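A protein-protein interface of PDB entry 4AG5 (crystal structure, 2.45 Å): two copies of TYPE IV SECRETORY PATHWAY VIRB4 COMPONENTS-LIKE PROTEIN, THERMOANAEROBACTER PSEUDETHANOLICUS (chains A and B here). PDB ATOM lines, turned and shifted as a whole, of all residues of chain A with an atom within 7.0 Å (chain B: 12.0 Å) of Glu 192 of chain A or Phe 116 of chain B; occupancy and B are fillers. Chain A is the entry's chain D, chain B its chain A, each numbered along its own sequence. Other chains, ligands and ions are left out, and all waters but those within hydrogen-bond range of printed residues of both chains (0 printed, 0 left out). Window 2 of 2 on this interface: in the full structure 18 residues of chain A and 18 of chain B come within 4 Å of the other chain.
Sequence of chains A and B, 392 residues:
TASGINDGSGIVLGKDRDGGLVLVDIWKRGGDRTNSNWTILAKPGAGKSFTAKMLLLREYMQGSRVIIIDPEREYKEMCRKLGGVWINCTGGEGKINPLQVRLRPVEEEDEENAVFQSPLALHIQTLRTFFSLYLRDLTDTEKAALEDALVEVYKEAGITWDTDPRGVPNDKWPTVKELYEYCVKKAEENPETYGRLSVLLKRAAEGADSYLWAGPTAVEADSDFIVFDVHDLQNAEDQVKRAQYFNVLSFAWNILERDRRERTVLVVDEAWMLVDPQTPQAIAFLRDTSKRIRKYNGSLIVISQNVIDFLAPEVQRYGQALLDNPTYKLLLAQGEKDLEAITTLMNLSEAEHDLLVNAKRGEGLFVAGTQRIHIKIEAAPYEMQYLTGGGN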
ATOM      1  N   THR A 139      20.941   3.138  -7.717  1.00  0.00           N
ATOM      2  CA  THR A 139      21.013   3.659  -9.075  1.00  0.00           C
ATOM      3  C   THR A 139      20.346   2.688 -10.034  1.00  0.00           C
ATOM      4  O   THR A 139      20.231   1.499  -9.726  1.00  0.00           O
ATOM      5  CB  THR A 139      22.471   3.863  -9.539  1.00  0.00           C
ATOM      6  OG1 THR A 139      23.130   2.591  -9.662  1.00  0.00           O
ATOM      7  CG2 THR A 139      23.230   4.752  -8.562  1.00  0.00           C
ATOM      8  N   ASP A 140      19.915   3.198 -11.192  1.00  0.00           N
ATOM      9  CA  ASP A 140      19.368   2.365 -12.263  1.00  0.00           C
ATOM     10  C   ASP A 140      20.317   1.223 -12.615  1.00  0.00           C
ATOM     11  O   ASP A 140      19.887   0.080 -12.800  1.00  0.00           O
ATOM     12  CB  ASP A 140      19.089   3.201 -13.517  1.00  0.00           C
ATOM     13  CG  ASP A 140      17.950   4.188 -13.327  1.00  0.00           C
ATOM     14  OD1 ASP A 140      16.996   3.875 -12.583  1.00  0.00           O
ATOM     15  OD2 ASP A 140      18.004   5.283 -13.931  1.00  0.00           O
ATOM     16  N   THR A 141      21.606   1.547 -12.721  1.00  0.00           N
ATOM     17  CA  THR A 141      22.646   0.555 -12.959  1.00  0.00           C
ATOM     18  C   THR A 141      22.670  -0.458 -11.819  1.00  0.00           C
ATOM     19  O   THR A 141      22.766  -1.658 -12.047  1.00  0.00           O
ATOM     20  CB  THR A 141      24.041   1.213 -13.085  1.00  0.00           C
ATOM     21  OG1 THR A 141      24.295   1.554 -14.451  1.00  0.00           O
ATOM     22  CG2 THR A 141      25.145   0.259 -12.612  1.00  0.00           C
ATOM     23  N   GLU A 142      22.574   0.021 -10.583  1.00  0.00           N
ATOM     24  CA  GLU A 142      22.602  -0.886  -9.442  1.00  0.00           C
ATOM     25  C   GLU A 142      21.345  -1.749  -9.394  1.00  0.00           C
ATOM     26  O   GLU A 142      21.400  -2.920  -9.028  1.00  0.00           O
ATOM     27  CB  GLU A 142      22.798  -0.112  -8.142  1.00  0.00           C
ATOM     28  CG  GLU A 142      24.181   0.499  -8.010  1.00  0.00           C
ATOM     29  CD  GLU A 142      24.284   1.426  -6.812  1.00  0.00           C
ATOM     30  OE1 GLU A 142      23.227   1.923  -6.361  1.00  0.00           O
ATOM     31  OE2 GLU A 142      25.415   1.654  -6.328  1.00  0.00           O
ATOM     32  N   ALA A 187      31.594  -8.322  -7.323  1.00  0.00           N
ATOM     33  CA  ALA A 187      32.079  -6.972  -7.037  1.00  0.00           C
ATOM     34  C   ALA A 187      33.587  -6.870  -7.135  1.00  0.00           C
ATOM     35  O   ALA A 187      34.134  -5.770  -7.211  1.00  0.00           O
ATOM     36  CB  ALA A 187      31.597  -6.492  -5.686  1.00  0.00           C
ATOM     37  N   GLU A 189      35.350  -7.916  -9.730  1.00  0.00           N
ATOM     38  CA  GLU A 189      35.608  -7.406 -11.077  1.00  0.00           C
ATOM     39  C   GLU A 189      34.732  -6.196 -11.412  1.00  0.00           C
ATOM     40  O   GLU A 189      35.090  -5.377 -12.249  1.00  0.00           O
ATOM     41  CB  GLU A 189      35.439  -8.505 -12.133  1.00  0.00           C
ATOM     42  CG  GLU A 189      34.149  -9.309 -12.003  1.00  0.00           C
ATOM     43  CD  GLU A 189      33.732  -9.976 -13.308  1.00  0.00           C
ATOM     44  OE1 GLU A 189      34.510  -9.917 -14.284  1.00  0.00           O
ATOM     45  OE2 GLU A 189      32.624 -10.555 -13.357  1.00  0.00           O
ATOM     46  N   ASN A 190      33.589  -6.081 -10.748  1.00  0.00           N
ATOM     47  CA  ASN A 190      32.678  -4.973 -11.010  1.00  0.00           C
ATOM     48  C   ASN A 190      32.370  -4.131  -9.772  1.00  0.00           C
ATOM     49  O   ASN A 190      31.214  -4.041  -9.359  1.00  0.00           O
ATOM     50  CB  ASN A 190      31.370  -5.496 -11.606  1.00  0.00           C
ATOM     51  CG  ASN A 190      31.575  -6.229 -12.914  1.00  0.00           C
ATOM     52  OD1 ASN A 190      31.268  -5.706 -13.989  1.00  0.00           O
ATOM     53  ND2 ASN A 190      32.089  -7.449 -12.834  1.00  0.00           N
ATOM     54  N   PRO A 191      33.397  -3.493  -9.186  1.00  0.00           N
ATOM     55  CA  PRO A 191      33.159  -2.708  -7.966  1.00  0.00           C
ATOM     56  C   PRO A 191      32.248  -1.511  -8.228  1.00  0.00           C
ATOM     57  O   PRO A 191      31.423  -1.162  -7.382  1.00  0.00           O
ATOM     58  CB  PRO A 191      34.565  -2.243  -7.561  1.00  0.00           C
ATOM     59  CG  PRO A 191      35.352  -2.274  -8.836  1.00  0.00           C
ATOM     60  CD  PRO A 191      34.801  -3.430  -9.626  1.00  0.00           C
ATOM     61  N   GLU A 192      32.399  -0.894  -9.394  1.00  0.00           N
ATOM     62  CA  GLU A 192      31.590   0.255  -9.773  1.00  0.00           C
ATOM     63  C   GLU A 192      30.106  -0.088  -9.757  1.00  0.00           C
ATOM     64  O   GLU A 192      29.273   0.715  -9.334  1.00  0.00           O
ATOM     65  CB  GLU A 192      31.988   0.743 -11.167  1.00  0.00           C
ATOM     66  CG  GLU A 192      33.420   1.238 -11.282  1.00  0.00           C
ATOM     67  CD  GLU A 192      33.620   2.613 -10.670  1.00  0.00           C
ATOM     68  OE1 GLU A 192      33.012   2.889  -9.614  1.00  0.00           O
ATOM     69  OE2 GLU A 192      34.392   3.413 -11.244  1.00  0.00           O
ATOM     70  N   THR A 193      29.788  -1.292 -10.213  1.00  0.00           N
ATOM     71  CA  THR A 193      28.404  -1.731 -10.333  1.00  0.00           C
ATOM     72  C   THR A 193      27.924  -2.565  -9.134  1.00  0.00           C
ATOM     73  O   THR A 193      26.724  -2.589  -8.834  1.00  0.00           O
ATOM     74  CB  THR A 193      28.197  -2.537 -11.631  1.00  0.00           C
ATOM     75  OG1 THR A 193      28.594  -1.747 -12.766  1.00  0.00           O
ATOM     76  CG2 THR A 193      26.747  -2.940 -11.788  1.00  0.00           C
ATOM     77  N   TYR A 194      28.857  -3.229  -8.442  1.00  0.00           N
ATOM     78  CA  TYR A 194      28.490  -4.192  -7.386  1.00  0.00           C
ATOM     79  C   TYR A 194      28.990  -3.919  -5.959  1.00  0.00           C
ATOM     80  O   TYR A 194      28.406  -4.407  -4.993  1.00  0.00           O
ATOM     81  CB  TYR A 194      28.885  -5.616  -7.793  1.00  0.00           C
ATOM     82  CG  TYR A 194      27.865  -6.288  -8.671  1.00  0.00           C
ATOM     83  CD1 TYR A 194      26.562  -6.479  -8.230  1.00  0.00           C
ATOM     84  CD2 TYR A 194      28.201  -6.731  -9.937  1.00  0.00           C
ATOM     85  CE1 TYR A 194      25.623  -7.093  -9.024  1.00  0.00           C
ATOM     86  CE2 TYR A 194      27.261  -7.345 -10.745  1.00  0.00           C
ATOM     87  CZ  TYR A 194      25.976  -7.523 -10.284  1.00  0.00           C
ATOM     88  OH  TYR A 194      25.050  -8.136 -11.091  1.00  0.00           O
ATOM     89  N   GLY A 195      30.069  -3.155  -5.830  1.00  0.00           N
ATOM     90  CA  GLY A 195      30.667  -2.875  -4.535  1.00  0.00           C
ATOM     91  C   GLY A 195      29.689  -2.420  -3.467  1.00  0.00           C
ATOM     92  O   GLY A 195      29.568  -3.050  -2.407  1.00  0.00           O
ATOM     93  N   ARG A 196      28.992  -1.327  -3.752  1.00  0.00           N
ATOM     94  CA  ARG A 196      28.038  -0.738  -2.820  1.00  0.00           C
ATOM     95  C   ARG A 196      26.783  -1.588  -2.654  1.00  0.00           C
ATOM     96  O   ARG A 196      26.138  -1.564  -1.605  1.00  0.00           O
ATOM     97  CB  ARG A 196      27.656   0.672  -3.267  1.00  0.00           C
ATOM     98  CG  ARG A 196      27.444   1.649  -2.128  1.00  0.00           C
ATOM     99  CD  ARG A 196      27.163   3.053  -2.637  1.00  0.00           C
ATOM    100  NE  ARG A 196      25.805   3.287  -3.148  1.00  0.00           N
ATOM    101  CZ  ARG A 196      24.753   2.485  -2.982  1.00  0.00           C
ATOM    102  NH1 ARG A 196      24.846   1.346  -2.308  1.00  0.00           N
ATOM    103  NH2 ARG A 196      23.582   2.836  -3.500  1.00  0.00           N
ATOM    104  N   VAL B 101      28.428  -2.119 -27.468  1.00  0.00           N
ATOM    105  CA  VAL B 101      27.924  -1.241 -26.411  1.00  0.00           C
ATOM    106  C   VAL B 101      28.351   0.190 -26.692  1.00  0.00           C
ATOM    107  O   VAL B 101      29.498   0.437 -27.090  1.00  0.00           O
ATOM    108  CB  VAL B 101      28.388  -1.698 -24.997  1.00  0.00           C
ATOM    109  CG1 VAL B 101      27.830  -0.785 -23.917  1.00  0.00           C
ATOM    110  CG2 VAL B 101      27.925  -3.116 -24.727  1.00  0.00           C
ATOM    111  N   ARG B 102      27.424   1.129 -26.522  1.00  0.00           N
ATOM    112  CA  ARG B 102      27.710   2.510 -26.883  1.00  0.00           C
ATOM    113  C   ARG B 102      28.013   3.353 -25.659  1.00  0.00           C
ATOM    114  O   ARG B 102      27.369   3.211 -24.618  1.00  0.00           O
ATOM    115  CB  ARG B 102      26.552   3.131 -27.660  1.00  0.00           C
ATOM    116  CG  ARG B 102      25.742   2.147 -28.476  1.00  0.00           C
ATOM    117  CD  ARG B 102      26.430   1.728 -29.759  1.00  0.00           C
ATOM    118  NE  ARG B 102      25.482   1.770 -30.871  1.00  0.00           N
ATOM    119  CZ  ARG B 102      25.278   0.786 -31.740  1.00  0.00           C
ATOM    120  NH1 ARG B 102      25.967  -0.345 -31.656  1.00  0.00           N
ATOM    121  NH2 ARG B 102      24.383   0.945 -32.708  1.00  0.00           N
ATOM    122  N   LEU B 103      29.003   4.229 -25.800  1.00  0.00           N
ATOM    123  CA  LEU B 103      29.389   5.167 -24.753  1.00  0.00           C
ATOM    124  C   LEU B 103      28.165   5.906 -24.203  1.00  0.00           C
ATOM    125  O   LEU B 103      27.163   6.062 -24.906  1.00  0.00           O
ATOM    126  CB  LEU B 103      30.432   6.147 -25.301  1.00  0.00           C
ATOM    127  CG  LEU B 103      31.587   5.467 -26.055  1.00  0.00           C
ATOM    128  CD1 LEU B 103      32.478   6.482 -26.766  1.00  0.00           C
ATOM    129  CD2 LEU B 103      32.407   4.594 -25.111  1.00  0.00           C
ATOM    130  N   ARG B 104      28.256   6.351 -22.951  1.00  0.00           N
ATOM    131  CA  ARG B 104      27.092   6.834 -22.197  1.00  0.00           C
ATOM    132  C   ARG B 104      26.566   8.192 -22.659  1.00  0.00           C
ATOM    133  O   ARG B 104      26.775   9.213 -22.001  1.00  0.00           O
ATOM    134  CB  ARG B 104      27.399   6.863 -20.693  1.00  0.00           C
ATOM    135  N   VAL B 115      25.833   9.247 -10.217  1.00  0.00           N
ATOM    136  CA  VAL B 115      27.171   9.573 -10.701  1.00  0.00           C
ATOM    137  C   VAL B 115      27.688   8.515 -11.671  1.00  0.00           C
ATOM    138  O   VAL B 115      27.696   8.740 -12.885  1.00  0.00           O
ATOM    139  CB  VAL B 115      28.175   9.728  -9.556  1.00  0.00           C
ATOM    140  N   PHE B 116      28.123   7.367 -11.151  1.00  0.00           N
ATOM    141  CA  PHE B 116      28.582   6.295 -12.030  1.00  0.00           C
ATOM    142  C   PHE B 116      27.436   5.525 -12.670  1.00  0.00           C
ATOM    143  O   PHE B 116      26.458   5.176 -12.003  1.00  0.00           O
ATOM    144  CB  PHE B 116      29.506   5.305 -11.329  1.00  0.00           C
ATOM    145  CG  PHE B 116      29.779   4.066 -12.150  1.00  0.00           C
ATOM    146  CD1 PHE B 116      28.931   2.968 -12.080  1.00  0.00           C
ATOM    147  CD2 PHE B 116      30.861   4.013 -13.015  1.00  0.00           C
ATOM    148  CE1 PHE B 116      29.160   1.839 -12.839  1.00  0.00           C
ATOM    149  CE2 PHE B 116      31.108   2.877 -13.776  1.00  0.00           C
ATOM    150  CZ  PHE B 116      30.248   1.789 -13.689  1.00  0.00           C
ATOM    151  N   GLN B 117      27.595   5.250 -13.966  1.00  0.00           N
ATOM    152  CA  GLN B 117      26.629   4.495 -14.757  1.00  0.00           C
ATOM    153  C   GLN B 117      27.290   3.398 -15.597  1.00  0.00           C
ATOM    154  O   GLN B 117      28.285   3.639 -16.282  1.00  0.00           O
ATOM    155  CB  GLN B 117      25.829   5.433 -15.658  1.00  0.00           C
ATOM    156  CG  GLN B 117      24.472   5.765 -15.096  1.00  0.00           C
ATOM    157  CD  GLN B 117      23.751   4.522 -14.631  1.00  0.00           C
ATOM    158  OE1 GLN B 117      23.582   4.297 -13.428  1.00  0.00           O
ATOM    159  NE2 GLN B 117      23.335   3.691 -15.583  1.00  0.00           N
ATOM    160  N   SER B 118      26.726   2.196 -15.537  1.00  0.00           N
ATOM    161  CA  SER B 118      27.270   1.041 -16.249  1.00  0.00           C
ATOM    162  C   SER B 118      26.948   1.114 -17.740  1.00  0.00           C
ATOM    163  O   SER B 118      25.786   1.027 -18.133  1.00  0.00           O
ATOM    164  CB  SER B 118      26.702  -0.254 -15.655  1.00  0.00           C
ATOM    165  OG  SER B 118      26.970  -1.363 -16.494  1.00  0.00           O
ATOM    166  N   PRO B 119      27.980   1.277 -18.577  1.00  0.00           N
ATOM    167  CA  PRO B 119      27.761   1.349 -20.024  1.00  0.00           C
ATOM    168  C   PRO B 119      26.883   0.184 -20.494  1.00  0.00           C
ATOM    169  O   PRO B 119      25.986   0.354 -21.329  1.00  0.00           O
ATOM    170  CB  PRO B 119      29.181   1.230 -20.594  1.00  0.00           C
ATOM    171  CG  PRO B 119      30.001   0.630 -19.467  1.00  0.00           C
ATOM    172  CD  PRO B 119      29.412   1.217 -18.242  1.00  0.00           C
ATOM    173  N   LEU B 120      27.124  -0.989 -19.921  1.00  0.00           N
ATOM    174  CA  LEU B 120      26.415  -2.191 -20.328  1.00  0.00           C
ATOM    175  C   LEU B 120      24.917  -2.111 -20.060  1.00  0.00           C
ATOM    176  O   LEU B 120      24.125  -2.456 -20.927  1.00  0.00           O
ATOM    177  CB  LEU B 120      27.032  -3.426 -19.666  1.00  0.00           C
ATOM    178  CG  LEU B 120      26.385  -4.785 -19.937  1.00  0.00           C
ATOM    179  CD1 LEU B 120      26.147  -4.989 -21.424  1.00  0.00           C
ATOM    180  CD2 LEU B 120      27.245  -5.905 -19.364  1.00  0.00           C
ATOM    181  N   ALA B 121      24.530  -1.652 -18.871  1.00  0.00           N
ATOM    182  CA  ALA B 121      23.110  -1.560 -18.502  1.00  0.00           C
ATOM    183  C   ALA B 121      22.377  -0.607 -19.423  1.00  0.00           C
ATOM    184  O   ALA B 121      21.257  -0.878 -19.866  1.00  0.00           O
ATOM    185  CB  ALA B 121      22.966  -1.082 -17.083  1.00  0.00           C
ATOM    186  N   LEU B 122      23.021   0.529 -19.669  1.00  0.00           N
ATOM    187  CA  LEU B 122      22.511   1.547 -20.561  1.00  0.00           C
ATOM    188  C   LEU B 122      22.209   0.945 -21.924  1.00  0.00           C
ATOM    189  O   LEU B 122      21.164   1.205 -22.509  1.00  0.00           O
ATOM    190  CB  LEU B 122      23.554   2.655 -20.712  1.00  0.00           C
ATOM    191  CG  LEU B 122      23.278   3.986 -20.013  1.00  0.00           C
ATOM    192  CD1 LEU B 122      22.284   3.822 -18.870  1.00  0.00           C
ATOM    193  CD2 LEU B 122      24.581   4.628 -19.533  1.00  0.00           C
ATOM    194  N   HIS B 123      23.128   0.129 -22.424  1.00  0.00           N
ATOM    195  CA  HIS B 123      23.014  -0.372 -23.779  1.00  0.00           C
ATOM    196  C   HIS B 123      22.025  -1.529 -23.900  1.00  0.00           C
ATOM    197  O   HIS B 123      21.554  -1.844 -25.007  1.00  0.00           O
ATOM    198  CB  HIS B 123      24.381  -0.768 -24.341  1.00  0.00           C
ATOM    199  CG  HIS B 123      24.338  -1.090 -25.798  1.00  0.00           C
ATOM    200  ND1 HIS B 123      24.136  -0.119 -26.760  1.00  0.00           N
ATOM    201  CD2 HIS B 123      24.402  -2.272 -26.451  1.00  0.00           C
ATOM    202  CE1 HIS B 123      24.107  -0.697 -27.951  1.00  0.00           C
ATOM    203  NE2 HIS B 123      24.266  -1.997 -27.796  1.00  0.00           N
ATOM    204  N   ILE B 159      32.945  -9.084 -21.662  1.00  0.00           N
ATOM    205  CA  ILE B 159      32.482  -7.756 -21.283  1.00  0.00           C
ATOM    206  C   ILE B 159      31.544  -7.842 -20.083  1.00  0.00           C
ATOM    207  O   ILE B 159      30.667  -8.692 -20.038  1.00  0.00           O
ATOM    208  CB  ILE B 159      31.855  -6.940 -22.474  1.00  0.00           C
ATOM    209  CG1 ILE B 159      30.429  -6.531 -22.157  1.00  0.00           C
ATOM    210  CG2 ILE B 159      31.972  -7.672 -23.806  1.00  0.00           C
ATOM    211  CD1 ILE B 159      30.265  -5.044 -22.077  1.00  0.00           C
ATOM    212  N   THR B 160      31.766  -6.981 -19.096  1.00  0.00           N
ATOM    213  CA  THR B 160      30.940  -6.968 -17.886  1.00  0.00           C
ATOM    214  C   THR B 160      30.454  -5.565 -17.545  1.00  0.00           C
ATOM    215  O   THR B 160      30.637  -4.633 -18.325  1.00  0.00           O
ATOM    216  CB  THR B 160      31.665  -7.574 -16.645  1.00  0.00           C
ATOM    217  OG1 THR B 160      33.061  -7.243 -16.680  1.00  0.00           O
ATOM    218  CG2 THR B 160      31.494  -9.096 -16.598  1.00  0.00           C
ATOM    219  N   TRP B 161      29.853  -5.431 -16.365  1.00  0.00           N
ATOM    220  CA  TRP B 161      29.126  -4.222 -15.978  1.00  0.00           C
ATOM    221  C   TRP B 161      30.000  -2.986 -15.855  1.00  0.00           C
ATOM    222  O   TRP B 161      29.532  -1.875 -16.048  1.00  0.00           O
ATOM    223  CB  TRP B 161      28.365  -4.455 -14.669  1.00  0.00           C
ATOM    224  CG  TRP B 161      27.400  -5.585 -14.769  1.00  0.00           C
ATOM    225  CD1 TRP B 161      27.684  -6.913 -14.668  1.00  0.00           C
ATOM    226  CD2 TRP B 161      25.994  -5.491 -15.008  1.00  0.00           C
ATOM    227  NE1 TRP B 161      26.542  -7.655 -14.831  1.00  0.00           N
ATOM    228  CE2 TRP B 161      25.488  -6.802 -15.038  1.00  0.00           C
ATOM    229  CE3 TRP B 161      25.114  -4.427 -15.211  1.00  0.00           C
ATOM    230  CZ2 TRP B 161      24.142  -7.075 -15.254  1.00  0.00           C
ATOM    231  CZ3 TRP B 161      23.775  -4.702 -15.425  1.00  0.00           C
ATOM    232  CH2 TRP B 161      23.303  -6.014 -15.443  1.00  0.00           C
ATOM    233  N   ASP B 162      31.267  -3.177 -15.530  1.00  0.00           N
ATOM    234  CA  ASP B 162      32.163  -2.048 -15.328  1.00  0.00           C
ATOM    235  C   ASP B 162      32.929  -1.748 -16.603  1.00  0.00           C
ATOM    236  O   ASP B 162      33.465  -0.649 -16.776  1.00  0.00           O
ATOM    237  CB  ASP B 162      33.141  -2.340 -14.186  1.00  0.00           C
ATOM    238  CG  ASP B 162      32.550  -2.057 -12.809  1.00  0.00           C
ATOM    239  OD1 ASP B 162      31.308  -2.055 -12.660  1.00  0.00           O
ATOM    240  OD2 ASP B 162      33.343  -1.836 -11.870  1.00  0.00           O
ATOM    241  N   THR B 163      32.962  -2.733 -17.499  1.00  0.00           N
ATOM    242  CA  THR B 163      33.747  -2.638 -18.729  1.00  0.00           C
ATOM    243  C   THR B 163      33.538  -1.323 -19.480  1.00  0.00           C
ATOM    244  O   THR B 163      32.406  -0.892 -19.703  1.00  0.00           O
ATOM    245  CB  THR B 163      33.479  -3.829 -19.672  1.00  0.00           C
ATOM    246  OG1 THR B 163      34.050  -5.023 -19.112  1.00  0.00           O
ATOM    247  CG2 THR B 163      34.104  -3.568 -21.030  1.00  0.00           C
ATOM    248  N   ASP B 164      34.646  -0.690 -19.852  1.00  0.00           N
ATOM    249  CA  ASP B 164      34.620   0.564 -20.587  1.00  0.00           C
ATOM    250  C   ASP B 164      34.697   0.308 -22.095  1.00  0.00           C
ATOM    251  O   ASP B 164      35.696  -0.200 -22.602  1.00  0.00           O
ATOM    252  CB  ASP B 164      35.774   1.458 -20.129  1.00  0.00           C
ATOM    253  CG  ASP B 164      35.824   2.774 -20.873  1.00  0.00           C
ATOM    254  OD1 ASP B 164      34.842   3.108 -21.577  1.00  0.00           O
ATOM    255  OD2 ASP B 164      36.856   3.472 -20.762  1.00  0.00           O
ATOM    256  N   PRO B 165      33.619   0.639 -22.812  1.00  0.00           N
ATOM    257  CA  PRO B 165      33.516   0.452 -24.260  1.00  0.00           C
ATOM    258  C   PRO B 165      34.727   0.992 -25.011  1.00  0.00           C
ATOM    259  O   PRO B 165      35.205   0.344 -25.941  1.00  0.00           O
ATOM    260  CB  PRO B 165      32.284   1.278 -24.612  1.00  0.00           C
ATOM    261  CG  PRO B 165      31.423   1.147 -23.412  1.00  0.00           C
ATOM    262  CD  PRO B 165      32.347   1.101 -22.227  1.00  0.00           C
ATOM    263  N   ARG B 166      35.217   2.161 -24.607  1.00  0.00           N
ATOM    264  CA  ARG B 166      36.313   2.819 -25.315  1.00  0.00           C
ATOM    265  C   ARG B 166      37.526   1.917 -25.509  1.00  0.00           C
ATOM    266  O   ARG B 166      38.306   2.106 -26.441  1.00  0.00           O
ATOM    267  CB  ARG B 166      36.726   4.109 -24.603  1.00  0.00           C
ATOM    268  CG  ARG B 166      35.875   5.318 -24.958  1.00  0.00           C
ATOM    269  CD  ARG B 166      36.407   6.587 -24.308  1.00  0.00           C
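Phe 116 of chain B touches two residues of chain A. No residue of chain B comes within 4 Å of Thr 139 of chain A. Thr 141 of chain A touches just these residues of chain B: Gln 117 (2.6 Å), Ser 118 (2.7 Å) and Ala 121 (3.96 Å). No residue of chain B comes within 4 Å of Ala 187 of chain A. Printed residues of chain B within 4 Å of Asn 190 of chain A: Thr 160, Trp 161 and Asp 162. Pro 191 of chain A touches one residue of chain B. Thr 193 of chain A touches four residues of chain B. Of the printed residues of chain B, Tyr 194 of chain A touches Trp 161 (3.97 Å). Printed residues of chain A within 4 Å of Ser 118 of chain B: Thr 141 (2.7 Å) and Thr 193 (3.8 Å). Printed residues of chain A within 4 Å of Asp 162 of chain B: Glu 189 (3.97 Å), Asn 190 (3.0 Å), Pro 191 (3.1 Å), Glu 192 (2.8 Å) and Thr 193 (2.7 Å). Printed residues of chain A within 4 Å of Thr 160 of chain B: Glu 189 and Asn 190. Printed residues of chain A within 4 Å of Ala 121 of chain B: Thr 141. Arg 196 of chain A touches none of the printed residues of chain B. Glu 142 of chain A touches none of the printed residues of chain B. The nearest residue of chain B that does not touch Glu 192 of chain A is Trp 161 of chain B (6.1 Å).
The side-chain hydroxyl (OG1) of Thr 141 of chain A lies within hydrogen-bond range of the side-chain amide nitrogen (NE2) of Gln 117 of chain B, 2.6 Å away. N of Glu 192 of chain A sits at hydrogen-bond distance from OD2 of Asp 162 of chain B. N of Pro 191 of chain A lies close to OD2 of Asp 162 of chain B, at 3.2 Å. The side-chain amide oxygen (OD1) of Asn 190 of chain A is in hydrogen-bond range of the backbone NH (N) of Asp 162 of chain B (3.0 Å). OD1 of Asp 162 of chain B is in hydrogen-bond range of OG1 of Thr 193 of chain A (2.7 Å). The side-chain hydroxyl (OG1) of Thr 193 of chain A lies close to the backbone carbonyl oxygen (O) of Trp 161 of chain B, at 3.4 Å. The backbone NH of Trp 161 of chain B lies within hydrogen-bond range of the side-chain amide oxygen of Asn 190 of chain A (2.8 Å). OG1 of Thr 141 of chain A lies within hydrogen-bond range of N of Ser 118 of chain B (2.7 Å).
Hydrophobic or aromatic side chains of chain A within 4 Å of the printed part of chain B: Pro 191 and Tyr 194. Of the 21 printed residues of chain B, 7 touch a printed residue of chain A. Among the printed residues, 16 pairs touch across the chains. Among the printed residues, no Asp or Glu carboxylate lies within 4 Å of a Lys or Arg side-chain nitrogen of the other chain.
The side-chain hydroxyl of Ser 118 of chain B sits at hydrogen-bond distance from the backbone carbonyl oxygen of Trp 161 of chain B, at 2.7 Å. OG1 of Thr 163 of chain B sits at hydrogen-bond distance from N of Thr 160 of chain B, at 3.0 Å. The backbone NH of Leu 120 of chain B sits close to the side-chain hydroxyl of Ser 118 of chain B, at 3.5 Å. OE2 of Glu 189 of chain A lies close to ND2 of Asn 190 of chain A (3.2 Å). The backbone NH of Ala 121 of chain B is in hydrogen-bond range of the side-chain hydroxyl of Ser 118 of chain B, at 3.4 Å.
No position is printed for both chains.
Among the printed residues, pairs that only touch across the chains: Thr 141 of chain A with Ala 121 of chain B (3.96 Å), Glu 189 of chain A with Thr 160 of chain B (3.7 Å), Glu 189 of chain A with Asp 162 of chain B (3.97 Å), Asn 190 of chain A with Thr 160 of chain B (3.3 Å), Glu 192 of chain A with Phe 116 of chain B (3.2 Å), Thr 193 of chain A with Phe 116 of chain B (3.6 Å), Thr 193 of chain A with Ser 118 of chain B (3.8 Å) and Tyr 194 of chain A with Trp 161 of chain B (3.97 Å).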
